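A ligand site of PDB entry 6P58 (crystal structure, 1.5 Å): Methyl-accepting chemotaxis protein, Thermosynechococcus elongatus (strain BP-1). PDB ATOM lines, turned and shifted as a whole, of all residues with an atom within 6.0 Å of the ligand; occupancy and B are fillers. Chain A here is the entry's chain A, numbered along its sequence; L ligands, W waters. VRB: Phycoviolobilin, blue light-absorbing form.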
ATOM      1  N   ILE A  27      -5.074  11.380  18.986  1.00  0.00           N
ATOM      2  CA  ILE A  27      -5.400  10.113  19.632  1.00  0.00           C
ATOM      3  C   ILE A  27      -6.145  10.369  20.932  1.00  0.00           C
ATOM      4  O   ILE A  27      -6.041  11.437  21.538  1.00  0.00           O
ATOM      5  CB  ILE A  27      -4.142   9.260  19.914  1.00  0.00           C
ATOM      6  CG1 ILE A  27      -3.146  10.034  20.779  1.00  0.00           C
ATOM      7  CG2 ILE A  27      -3.507   8.816  18.607  1.00  0.00           C
ATOM      8  CD1 ILE A  27      -1.970   9.201  21.258  1.00  0.00           C
ATOM      9  N   TYR A  29      -5.980   8.656  24.590  1.00  0.00           N
ATOM     10  CA  TYR A  29      -5.069   7.864  25.403  1.00  0.00           C
ATOM     11  C   TYR A  29      -5.763   7.656  26.742  1.00  0.00           C
ATOM     12  O   TYR A  29      -5.881   8.583  27.536  1.00  0.00           O
ATOM     13  CB  TYR A  29      -3.762   8.645  25.545  1.00  0.00           C
ATOM     14  CG  TYR A  29      -2.634   8.033  26.359  1.00  0.00           C
ATOM     15  CD1 TYR A  29      -1.874   6.977  25.867  1.00  0.00           C
ATOM     16  CD2 TYR A  29      -2.301   8.550  27.595  1.00  0.00           C
ATOM     17  CE1 TYR A  29      -0.823   6.443  26.611  1.00  0.00           C
ATOM     18  CE2 TYR A  29      -1.263   8.033  28.335  1.00  0.00           C
ATOM     19  CZ  TYR A  29      -0.522   6.987  27.844  1.00  0.00           C
ATOM     20  OH  TYR A  29       0.509   6.465  28.588  1.00  0.00           O
ATOM     21  N   VAL A  39      -3.765   3.638  23.598  1.00  0.00           N
ATOM     22  CA  VAL A  39      -4.288   4.413  22.484  1.00  0.00           C
ATOM     23  C   VAL A  39      -5.521   3.694  21.973  1.00  0.00           C
ATOM     24  O   VAL A  39      -5.427   2.625  21.365  1.00  0.00           O
ATOM     25  CB  VAL A  39      -3.238   4.592  21.384  1.00  0.00           C
ATOM     26  CG1 VAL A  39      -3.781   5.496  20.285  1.00  0.00           C
ATOM     27  CG2 VAL A  39      -1.952   5.161  21.960  1.00  0.00           C
ATOM     28  N   ILE A  56       1.043   2.018  26.338  1.00  0.00           N
ATOM     29  CA  ILE A  56       2.250   2.777  26.668  1.00  0.00           C
ATOM     30  C   ILE A  56       2.183   3.099  28.159  1.00  0.00           C
ATOM     31  O   ILE A  56       1.365   3.927  28.579  1.00  0.00           O
ATOM     32  CB  ILE A  56       2.380   4.056  25.836  1.00  0.00           C
ATOM     33  CG1 ILE A  56       2.356   3.728  24.341  1.00  0.00           C
ATOM     34  CG2 ILE A  56       3.655   4.815  26.215  1.00  0.00           C
ATOM     35  CD1 ILE A  56       2.158   4.934  23.457  1.00  0.00           C
ATOM     36  N   GLU A  57       3.051   2.473  28.942  1.00  0.00           N
ATOM     37  CA  GLU A  57       3.125   2.749  30.378  1.00  0.00           C
ATOM     38  C   GLU A  57       4.154   3.850  30.615  1.00  0.00           C
ATOM     39  O   GLU A  57       5.349   3.641  30.402  1.00  0.00           O
ATOM     40  CB  GLU A  57       3.493   1.496  31.165  1.00  0.00           C
ATOM     41  CG  GLU A  57       3.795   1.821  32.613  1.00  0.00           C
ATOM     42  CD  GLU A  57       3.843   0.604  33.501  1.00  0.00           C
ATOM     43  OE1 GLU A  57       4.045  -0.517  32.977  1.00  0.00           O
ATOM     44  OE2 GLU A  57       3.682   0.766  34.728  1.00  0.00           O
ATOM     45  N   ASP A  58       3.678   4.989  31.075  1.00  0.00           N
ATOM     46  CA  ASP A  58       4.544   6.134  31.375  1.00  0.00           C
ATOM     47  C   ASP A  58       4.295   6.525  32.831  1.00  0.00           C
ATOM     48  O   ASP A  58       3.222   7.067  33.138  1.00  0.00           O
ATOM     49  CB  ASP A  58       4.229   7.288  30.435  1.00  0.00           C
ATOM     50  CG  ASP A  58       5.220   8.422  30.554  1.00  0.00           C
ATOM     51  OD1 ASP A  58       5.859   8.546  31.619  1.00  0.00           O
ATOM     52  OD2 ASP A  58       5.363   9.190  29.577  1.00  0.00           O
ATOM     53  N   PRO A  59       5.234   6.277  33.738  1.00  0.00           N
ATOM     54  CA  PRO A  59       4.948   6.494  35.171  1.00  0.00           C
ATOM     55  C   PRO A  59       4.815   7.959  35.573  1.00  0.00           C
ATOM     56  O   PRO A  59       4.328   8.215  36.683  1.00  0.00           O
ATOM     57  CB  PRO A  59       6.149   5.837  35.881  1.00  0.00           C
ATOM     58  CG  PRO A  59       7.252   5.873  34.876  1.00  0.00           C
ATOM     59  CD  PRO A  59       6.593   5.745  33.523  1.00  0.00           C
ATOM     60  N   CYS A  60       5.208   8.909  34.723  1.00  0.00           N
ATOM     61  CA  CYS A  60       5.199  10.300  35.168  1.00  0.00           C
ATOM     62  C   CYS A  60       3.797  10.781  35.523  1.00  0.00           C
ATOM     63  O   CYS A  60       3.640  11.633  36.397  1.00  0.00           O
ATOM     64  CB  CYS A  60       5.836  11.209  34.105  1.00  0.00           C
ATOM     65  SG  CYS A  60       4.781  11.618  32.679  1.00  0.00           S
ATOM     66  N   PHE A  61       2.762  10.235  34.883  1.00  0.00           N
ATOM     67  CA  PHE A  61       1.405  10.693  35.155  1.00  0.00           C
ATOM     68  C   PHE A  61       0.992  10.348  36.577  1.00  0.00           C
ATOM     69  O   PHE A  61       0.635  11.233  37.370  1.00  0.00           O
ATOM     70  CB  PHE A  61       0.440  10.098  34.130  1.00  0.00           C
ATOM     71  CG  PHE A  61       0.668  10.589  32.731  1.00  0.00           C
ATOM     72  CD1 PHE A  61       0.367  11.891  32.380  1.00  0.00           C
ATOM     73  CD2 PHE A  61       1.209   9.743  31.775  1.00  0.00           C
ATOM     74  CE1 PHE A  61       0.582  12.349  31.103  1.00  0.00           C
ATOM     75  CE2 PHE A  61       1.431  10.205  30.492  1.00  0.00           C
ATOM     76  CZ  PHE A  61       1.125  11.507  30.155  1.00  0.00           C
ATOM     77  N   GLU A  63       2.811   9.466  39.020  1.00  0.00           N
ATOM     78  CA  GLU A  63       3.759   9.929  40.030  1.00  0.00           C
ATOM     79  C   GLU A  63       3.703  11.438  40.253  1.00  0.00           C
ATOM     80  O   GLU A  63       4.040  11.899  41.344  1.00  0.00           O
ATOM     81  CB  GLU A  63       5.178   9.492  39.640  1.00  0.00           C
ATOM     82  CG  GLU A  63       5.409   8.001  39.801  1.00  0.00           C
ATOM     83  CD  GLU A  63       6.826   7.575  39.463  1.00  0.00           C
ATOM     84  OE1 GLU A  63       7.688   8.463  39.278  1.00  0.00           O
ATOM     85  OE2 GLU A  63       7.076   6.351  39.383  1.00  0.00           O
ATOM     86  N   HIS A  64       3.261  12.212  39.253  1.00  0.00           N
ATOM     87  CA  HIS A  64       3.379  13.663  39.371  1.00  0.00           C
ATOM     88  C   HIS A  64       2.122  14.425  38.971  1.00  0.00           C
ATOM     89  O   HIS A  64       1.845  15.469  39.576  1.00  0.00           O
ATOM     90  CB  HIS A  64       4.541  14.174  38.505  1.00  0.00           C
ATOM     91  CG  HIS A  64       5.872  13.603  38.876  1.00  0.00           C
ATOM     92  ND1 HIS A  64       6.296  13.502  40.187  1.00  0.00           N
ATOM     93  CD2 HIS A  64       6.876  13.108  38.121  1.00  0.00           C
ATOM     94  CE1 HIS A  64       7.500  12.960  40.216  1.00  0.00           C
ATOM     95  NE2 HIS A  64       7.876  12.715  38.975  1.00  0.00           N
ATOM     96  N   TRP A  65       1.361  13.968  37.970  1.00  0.00           N
ATOM     97  CA  TRP A  65       0.495  14.871  37.219  1.00  0.00           C
ATOM     98  C   TRP A  65      -0.981  14.526  37.188  1.00  0.00           C
ATOM     99  O   TRP A  65      -1.760  15.331  36.661  1.00  0.00           O
ATOM    100  CB  TRP A  65       1.001  14.999  35.767  1.00  0.00           C
ATOM    101  CG  TRP A  65       2.442  15.382  35.688  1.00  0.00           C
ATOM    102  CD1 TRP A  65       3.441  14.683  35.063  1.00  0.00           C
ATOM    103  CD2 TRP A  65       3.060  16.537  36.250  1.00  0.00           C
ATOM    104  NE1 TRP A  65       4.631  15.344  35.193  1.00  0.00           N
ATOM    105  CE2 TRP A  65       4.430  16.488  35.923  1.00  0.00           C
ATOM    106  CE3 TRP A  65       2.593  17.624  37.005  1.00  0.00           C
ATOM    107  CZ2 TRP A  65       5.333  17.468  36.333  1.00  0.00           C
ATOM    108  CZ3 TRP A  65       3.490  18.596  37.397  1.00  0.00           C
ATOM    109  CH2 TRP A  65       4.844  18.517  37.055  1.00  0.00           C
ATOM    110  N   TYR A  69      -3.803  17.235  35.991  1.00  0.00           N
ATOM    111  CA  TYR A  69      -4.602  17.084  34.782  1.00  0.00           C
ATOM    112  C   TYR A  69      -6.091  17.104  35.100  1.00  0.00           C
ATOM    113  O   TYR A  69      -6.892  17.657  34.331  1.00  0.00           O
ATOM    114  CB  TYR A  69      -4.204  15.807  34.043  1.00  0.00           C
ATOM    115  CG  TYR A  69      -3.043  16.026  33.085  1.00  0.00           C
ATOM    116  CD1 TYR A  69      -3.230  16.722  31.896  1.00  0.00           C
ATOM    117  CD2 TYR A  69      -1.775  15.542  33.376  1.00  0.00           C
ATOM    118  CE1 TYR A  69      -2.173  16.931  31.019  1.00  0.00           C
ATOM    119  CE2 TYR A  69      -0.718  15.743  32.514  1.00  0.00           C
ATOM    120  CZ  TYR A  69      -0.923  16.441  31.341  1.00  0.00           C
ATOM    121  OH  TYR A  69       0.120  16.653  30.467  1.00  0.00           O
ATOM    122  N   ARG A  73      -4.673  20.932  33.761  1.00  0.00           N
ATOM    123  CA  ARG A  73      -3.329  21.027  33.205  1.00  0.00           C
ATOM    124  C   ARG A  73      -3.325  20.552  31.758  1.00  0.00           C
ATOM    125  O   ARG A  73      -4.094  19.655  31.373  1.00  0.00           O
ATOM    126  CB  ARG A  73      -2.374  20.169  34.023  1.00  0.00           C
ATOM    127  CG  ARG A  73      -0.911  20.219  33.601  1.00  0.00           C
ATOM    128  CD  ARG A  73      -0.140  19.094  34.266  1.00  0.00           C
ATOM    129  NE  ARG A  73       1.288  19.109  33.972  1.00  0.00           N
ATOM    130  CZ  ARG A  73       2.163  19.936  34.529  1.00  0.00           C
ATOM    131  NH1 ARG A  73       1.769  20.848  35.401  1.00  0.00           N
ATOM    132  NH2 ARG A  73       3.453  19.852  34.208  1.00  0.00           N
ATOM    133  N   ILE A  74      -2.463  21.155  30.951  1.00  0.00           N
ATOM    134  CA  ILE A  74      -2.184  20.669  29.598  1.00  0.00           C
ATOM    135  C   ILE A  74      -0.685  20.431  29.468  1.00  0.00           C
ATOM    136  O   ILE A  74       0.085  20.736  30.388  1.00  0.00           O
ATOM    137  CB  ILE A  74      -2.684  21.650  28.520  1.00  0.00           C
ATOM    138  CG1 ILE A  74      -1.874  22.954  28.534  1.00  0.00           C
ATOM    139  CG2 ILE A  74      -4.164  21.944  28.721  1.00  0.00           C
ATOM    140  CD1 ILE A  74      -2.147  23.836  27.331  1.00  0.00           C
ATOM    141  N   GLN A  75      -0.266  19.896  28.325  1.00  0.00           N
ATOM    142  CA  GLN A  75       1.130  19.946  27.900  1.00  0.00           C
ATOM    143  C   GLN A  75       1.144  20.458  26.474  1.00  0.00           C
ATOM    144  O   GLN A  75       0.540  19.841  25.591  1.00  0.00           O
ATOM    145  CB  GLN A  75       1.815  18.581  27.982  1.00  0.00           C
ATOM    146  CG  GLN A  75       3.204  18.534  27.330  1.00  0.00           C
ATOM    147  CD  GLN A  75       4.295  19.089  28.210  1.00  0.00           C
ATOM    148  OE1 GLN A  75       4.710  18.453  29.178  1.00  0.00           O
ATOM    149  NE2 GLN A  75       4.785  20.285  27.879  1.00  0.00           N
ATOM    150  N   LEU A  85      14.243  16.170  27.470  1.00  0.00           N
ATOM    151  CA  LEU A  85      13.629  14.916  27.910  1.00  0.00           C
ATOM    152  C   LEU A  85      14.668  13.803  27.966  1.00  0.00           C
ATOM    153  O   LEU A  85      15.689  13.824  27.277  1.00  0.00           O
ATOM    154  CB  LEU A  85      12.497  14.532  26.963  1.00  0.00           C
ATOM    155  CG  LEU A  85      11.365  15.561  26.859  1.00  0.00           C
ATOM    156  CD1 LEU A  85      10.557  15.362  25.583  1.00  0.00           C
ATOM    157  CD2 LEU A  85      10.459  15.497  28.081  1.00  0.00           C
ATOM    158  N   THR A  86      14.380  12.804  28.808  1.00  0.00           N
ATOM    159  CA  THR A  86      15.275  11.673  28.983  1.00  0.00           C
ATOM    160  C   THR A  86      15.151  10.715  27.808  1.00  0.00           C
ATOM    161  O   THR A  86      14.203  10.753  27.022  1.00  0.00           O
ATOM    162  CB  THR A  86      14.932  10.927  30.272  1.00  0.00           C
ATOM    163  OG1 THR A  86      13.648  10.308  30.140  1.00  0.00           O
ATOM    164  CG2 THR A  86      14.911  11.891  31.453  1.00  0.00           C
ATOM    165  N   CYS A  88      14.463   7.636  28.027  1.00  0.00           N
ATOM    166  CA  CYS A  88      13.260   6.840  28.248  1.00  0.00           C
ATOM    167  C   CYS A  88      12.056   7.479  27.581  1.00  0.00           C
ATOM    168  O   CYS A  88      11.231   6.793  26.968  1.00  0.00           O
ATOM    169  CB  CYS A  88      13.000   6.656  29.744  1.00  0.00           C
ATOM    170  SG  CYS A  88      11.755   5.387  30.104  1.00  0.00           S
ATOM    171  N   HIS A  89      11.904   8.798  27.749  1.00  0.00           N
ATOM    172  CA  HIS A  89      10.760   9.492  27.176  1.00  0.00           C
ATOM    173  C   HIS A  89      10.843   9.509  25.650  1.00  0.00           C
ATOM    174  O   HIS A  89       9.870   9.178  24.962  1.00  0.00           O
ATOM    175  CB  HIS A  89      10.676  10.915  27.731  1.00  0.00           C
ATOM    176  CG  HIS A  89       9.411  11.622  27.394  1.00  0.00           C
ATOM    177  ND1 HIS A  89       8.521  12.058  28.346  1.00  0.00           N
ATOM    178  CD2 HIS A  89       8.877  11.985  26.199  1.00  0.00           C
ATOM    179  CE1 HIS A  89       7.499  12.650  27.761  1.00  0.00           C
ATOM    180  NE2 HIS A  89       7.691  12.624  26.462  1.00  0.00           N
ATOM    181  N   GLN A  92       9.909   6.117  23.965  1.00  0.00           N
ATOM    182  CA  GLN A  92       8.523   5.704  23.837  1.00  0.00           C
ATOM    183  C   GLN A  92       7.804   6.456  22.723  1.00  0.00           C
ATOM    184  O   GLN A  92       6.813   5.944  22.193  1.00  0.00           O
ATOM    185  CB  GLN A  92       7.790   5.849  25.173  1.00  0.00           C
ATOM    186  CG  GLN A  92       7.295   7.249  25.497  1.00  0.00           C
ATOM    187  CD  GLN A  92       6.897   7.399  26.959  1.00  0.00           C
ATOM    188  OE1 GLN A  92       6.712   6.411  27.674  1.00  0.00           O
ATOM    189  NE2 GLN A  92       6.757   8.638  27.400  1.00  0.00           N
ATOM    190  N   LEU A  93       8.277   7.644  22.356  1.00  0.00           N
ATOM    191  CA  LEU A  93       7.684   8.394  21.251  1.00  0.00           C
ATOM    192  C   LEU A  93       8.310   8.073  19.903  1.00  0.00           C
ATOM    193  O   LEU A  93       7.678   8.322  18.869  1.00  0.00           O
ATOM    194  CB  LEU A  93       7.855   9.902  21.499  1.00  0.00           C
ATOM    195  CG  LEU A  93       7.226  10.462  22.784  1.00  0.00           C
ATOM    196  CD1 LEU A  93       7.443  11.967  22.859  1.00  0.00           C
ATOM    197  CD2 LEU A  93       5.751  10.130  22.861  1.00  0.00           C
ATOM    198  N   LEU A  96       6.350   6.304  17.114  1.00  0.00           N
ATOM    199  CA  LEU A  96       5.166   7.029  16.641  1.00  0.00           C
ATOM    200  C   LEU A  96       5.527   8.219  15.770  1.00  0.00           C
ATOM    201  O   LEU A  96       4.735   8.599  14.895  1.00  0.00           O
ATOM    202  CB  LEU A  96       4.342   7.520  17.834  1.00  0.00           C
ATOM    203  CG  LEU A  96       3.809   6.466  18.807  1.00  0.00           C
ATOM    204  CD1 LEU A  96       2.776   7.080  19.732  1.00  0.00           C
ATOM    205  CD2 LEU A  96       3.222   5.277  18.058  1.00  0.00           C
ATOM    206  N   VAL A  98       6.975  11.885  16.891  1.00  0.00           N
ATOM    207  CA  VAL A  98       6.406  13.052  17.559  1.00  0.00           C
ATOM    208  C   VAL A  98       7.494  14.118  17.613  1.00  0.00           C
ATOM    209  O   VAL A  98       8.544  13.900  18.223  1.00  0.00           O
ATOM    210  CB  VAL A  98       5.939  12.719  18.991  1.00  0.00           C
ATOM    211  CG1 VAL A  98       5.306  13.948  19.639  1.00  0.00           C
ATOM    212  CG2 VAL A  98       4.949  11.570  18.970  1.00  0.00           C
ATOM    213  N   ASN A 101       3.782  18.255  20.480  1.00  0.00           N
ATOM    214  CA  ASN A 101       2.547  17.635  20.950  1.00  0.00           C
ATOM    215  C   ASN A 101       1.741  18.579  21.826  1.00  0.00           C
ATOM    216  O   ASN A 101       2.266  19.530  22.418  1.00  0.00           O
ATOM    217  CB  ASN A 101       2.789  16.274  21.630  1.00  0.00           C
ATOM    218  CG  ASN A 101       3.675  16.341  22.852  1.00  0.00           C
ATOM    219  OD1 ASN A 101       4.168  17.407  23.219  1.00  0.00           O
ATOM    220  ND2 ASN A 101       3.886  15.204  23.496  1.00  0.00           N
ATOM    221  N   VAL A 103      -1.381  18.083  24.702  1.00  0.00           N
ATOM    222  CA  VAL A 103      -2.033  17.089  25.558  1.00  0.00           C
ATOM    223  C   VAL A 103      -3.072  17.820  26.396  1.00  0.00           C
ATOM    224  O   VAL A 103      -2.736  18.770  27.113  1.00  0.00           O
ATOM    225  CB  VAL A 103      -1.010  16.393  26.464  1.00  0.00           C
ATOM    226  CG1 VAL A 103      -1.685  15.364  27.355  1.00  0.00           C
ATOM    227  CG2 VAL A 103       0.109  15.778  25.640  1.00  0.00           C
ATOM    228  N   ILE A 117      -4.723  13.882  22.633  1.00  0.00           N
ATOM    229  CA  ILE A 117      -3.346  14.250  22.317  1.00  0.00           C
ATOM    230  C   ILE A 117      -3.224  14.482  20.818  1.00  0.00           C
ATOM    231  O   ILE A 117      -3.652  13.659  20.012  1.00  0.00           O
ATOM    232  CB  ILE A 117      -2.346  13.177  22.777  1.00  0.00           C
ATOM    233  CG1 ILE A 117      -2.489  12.943  24.284  1.00  0.00           C
ATOM    234  CG2 ILE A 117      -0.924  13.582  22.419  1.00  0.00           C
ATOM    235  CD1 ILE A 117      -1.557  11.894  24.855  1.00  0.00           C
ATOM    236  N   ALA A 118      -2.609  15.611  20.446  1.00  0.00           N
ATOM    237  CA  ALA A 118      -2.301  15.939  19.075  1.00  0.00           C
ATOM    238  C   ALA A 118      -0.794  15.896  18.876  1.00  0.00           C
ATOM    239  O   ALA A 118      -0.033  16.345  19.732  1.00  0.00           O
ATOM    240  CB  ALA A 118      -2.817  17.344  18.718  1.00  0.00           C
ATOM    241  N   HIS A 119      -0.368  15.366  17.728  1.00  0.00           N
ATOM    242  CA  HIS A 119       1.033  15.292  17.358  1.00  0.00           C
ATOM    243  C   HIS A 119       1.264  15.993  16.032  1.00  0.00           C
ATOM    244  O   HIS A 119       0.477  15.851  15.100  1.00  0.00           O
ATOM    245  CB  HIS A 119       1.491  13.832  17.176  1.00  0.00           C
ATOM    246  CG  HIS A 119       1.521  13.032  18.436  1.00  0.00           C
ATOM    247  ND1 HIS A 119       1.387  11.662  18.445  1.00  0.00           N
ATOM    248  CD2 HIS A 119       1.676  13.400  19.726  1.00  0.00           C
ATOM    249  CE1 HIS A 119       1.454  11.219  19.678  1.00  0.00           C
ATOM    250  NE2 HIS A 119       1.633  12.249  20.485  1.00  0.00           N
HETATM  251  C01 VRB L   1       8.975   5.707  30.075  1.00  0.00           C
HETATM  252  C02 VRB L   1      10.317   6.311  30.447  1.00  0.00           C
HETATM  253  C03 VRB L   1      10.320   7.098  31.726  1.00  0.00           C
HETATM  254  C04 VRB L   1      10.317   6.540  32.919  1.00  0.00           C
HETATM  255  C05 VRB L   1      10.303   5.067  33.247  1.00  0.00           C
HETATM  256  C06 VRB L   1      10.277   7.674  33.845  1.00  0.00           C
HETATM  257  O07 VRB L   1      10.265   7.495  35.049  1.00  0.00           O
HETATM  258  N08 VRB L   1      10.263   8.878  33.227  1.00  0.00           N
HETATM  259  C09 VRB L   1      10.319   8.608  31.772  1.00  0.00           C
HETATM  260  C10 VRB L   1       9.129   9.096  30.966  1.00  0.00           C
HETATM  261  C11 VRB L   1       8.678  10.496  31.253  1.00  0.00           C
HETATM  262  C12 VRB L   1       9.388  11.645  31.426  1.00  0.00           C
HETATM  263  C13 VRB L   1      10.890  11.802  31.387  1.00  0.00           C
HETATM  264  C14 VRB L   1       8.474  12.686  31.640  1.00  0.00           C
HETATM  265  C15 VRB L   1       7.193  12.114  31.587  1.00  0.00           C
HETATM  266  C16 VRB L   1       5.806  12.809  31.770  1.00  0.00           C
HETATM  267  C17 VRB L   1       5.022  12.827  30.410  1.00  0.00           C
HETATM  268  C18 VRB L   1       4.419  13.954  29.807  1.00  0.00           C
HETATM  269  C19 VRB L   1       4.472  15.346  30.382  1.00  0.00           C
HETATM  270  C20 VRB L   1       3.487  15.474  31.539  1.00  0.00           C
HETATM  271  C21 VRB L   1       3.327  16.907  31.998  1.00  0.00           C
HETATM  272  O22 VRB L   1       2.148  17.512  31.876  1.00  0.00           O
HETATM  273  O23 VRB L   1       4.275  17.492  32.486  1.00  0.00           O
HETATM  274  C24 VRB L   1       3.836  13.506  28.647  1.00  0.00           C
HETATM  275  C25 VRB L   1       4.099  12.111  28.562  1.00  0.00           C
HETATM  276  N26 VRB L   1       4.792  11.767  29.643  1.00  0.00           N
HETATM  277  C27 VRB L   1       3.709  11.074  27.593  1.00  0.00           C
HETATM  278  C28 VRB L   1       3.209  11.200  26.315  1.00  0.00           C
HETATM  279  N29 VRB L   1       3.312  12.242  25.383  1.00  0.00           N
HETATM  280  C30 VRB L   1       2.658  11.865  24.268  1.00  0.00           C
HETATM  281  O31 VRB L   1       2.534  12.532  23.245  1.00  0.00           O
HETATM  282  C32 VRB L   1       2.121  10.575  24.463  1.00  0.00           C
HETATM  283  C33 VRB L   1       2.461  10.163  25.703  1.00  0.00           C
HETATM  284  C34 VRB L   1       2.109   8.850  26.344  1.00  0.00           C
HETATM  285  C35 VRB L   1       1.309   9.794  23.455  1.00  0.00           C
HETATM  286  C36 VRB L   1       2.234   8.983  22.540  1.00  0.00           C
HETATM  287  C37 VRB L   1       3.078  14.363  27.668  1.00  0.00           C
HETATM  288  N38 VRB L   1       7.345  10.788  31.343  1.00  0.00           N
HETATM  289  C39 VRB L   1       8.759  14.132  31.904  1.00  0.00           C
HETATM  290  C40 VRB L   1       9.255  14.321  33.335  1.00  0.00           C
HETATM  291  C41 VRB L   1       8.102  14.262  34.297  1.00  0.00           C
HETATM  292  O42 VRB L   1       7.114  14.939  34.130  1.00  0.00           O
HETATM  293  O43 VRB L   1       8.175  13.418  35.336  1.00  0.00           O
HETATM  294  O   HOH W   1      12.279  10.857  34.808  1.00  0.00           O
HETATM  295  O   HOH W   2       6.839  17.163  32.971  1.00  0.00           O
HETATM  296  O   HOH W   3       5.763  14.420  25.558  1.00  0.00           O
HETATM  297  O   HOH W   4      13.259   9.065  32.526  1.00  0.00           O
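Water W4 lies within hydrogen-bond range of the side-chain hydroxyl of Thr 86 and a nitrogen (N08) of the ligand. Water W3 lies within hydrogen-bond range of NE2 of His 89, ND2 of Asn 101 and N29 of the ligand.
The side-chain sulfur (SG) of Cys 88 is covalently linked to a carbon (C02) of the ligand, at 1.7 Å. A carbon (C16) of the ligand is bonded to the side-chain sulfur (SG) of Cys 60 (1.8 Å). An oxygen (O22) of the ligand sits at hydrogen-bond distance from the side-chain hydroxyl (OH) of Tyr 69 (2.6 Å). The side-chain carboxylate of Asp 58 sits at hydrogen-bond distance from a nitrogen (N26) of the ligand (2.6 Å). The indole nitrogen of Trp 65 sits at hydrogen-bond distance from an oxygen (O42) of the ligand (2.7 Å). NE of Arg 73 lies within salt-bridge range of O22 of the ligand, at 2.8 Å. A ring nitrogen (NE2) of His 119 sits at hydrogen-bond distance from an oxygen (O31) of the ligand, 2.9 Å away. ND2 of Asn 101 is in hydrogen-bond range of O31 of the ligand (3.0 Å). A nitrogen (N38) of the ligand lies close to a ring nitrogen (ND1) of His 89 (3.5 Å). An oxygen (O23) of the ligand sits close to the side-chain amide oxygen (OE1) of Gln 75 (3.5 Å).
The backbone NH (N) of Cys 60 lies close to the side-chain carboxylate (OD1) of Asp 58, at 3.2 Å. The side-chain carboxylate (OD2) of Asp 58 sits at hydrogen-bond distance from the side-chain amide nitrogen (NE2) of Gln 92, 2.6 Å away. The backbone NH (N) of His 89 lies within hydrogen-bond range of the side-chain hydroxyl (OG1) of Thr 86 (3.3 Å). The backbone carbonyl oxygen (O) of Gln 75 sits at hydrogen-bond distance from the backbone NH (N) of Val 103. The side-chain hydroxyl of Tyr 29 sits at hydrogen-bond distance from the backbone carbonyl oxygen of Ile 56, at 2.7 Å. O of Ile 117 sits at hydrogen-bond distance from N of Ile 27.
Ile 27 touches the ligand. Tyr 29 touches the ligand. Pro 59 touches the ligand. Phe 61 touches the ligand (CZ to C25, 3.4 Å). CD2 of His 64 touches O43 of the ligand (3.1 Å). Thr 86 touches the ligand. OE1 of Gln 92 touches C01 of the ligand, at 3.4 Å. Leu 93 touches the ligand (CD2 to C36, 3.7 Å). CD1 of Leu 96 touches C36 of the ligand, 3.4 Å away. Val 103 touches the ligand (CG2 to C37, 3.9 Å). Ile 117 touches the ligand (CG2 to O31, 3.7 Å). Hydrophobic or aromatic side chains within 4 Å of the ligand: Ile 27, Tyr 29, Pro 59, Phe 61, His 64, Trp 65, Tyr 69, His 89, Leu 93, Leu 96, Val 103, Ile 117 and His 119.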
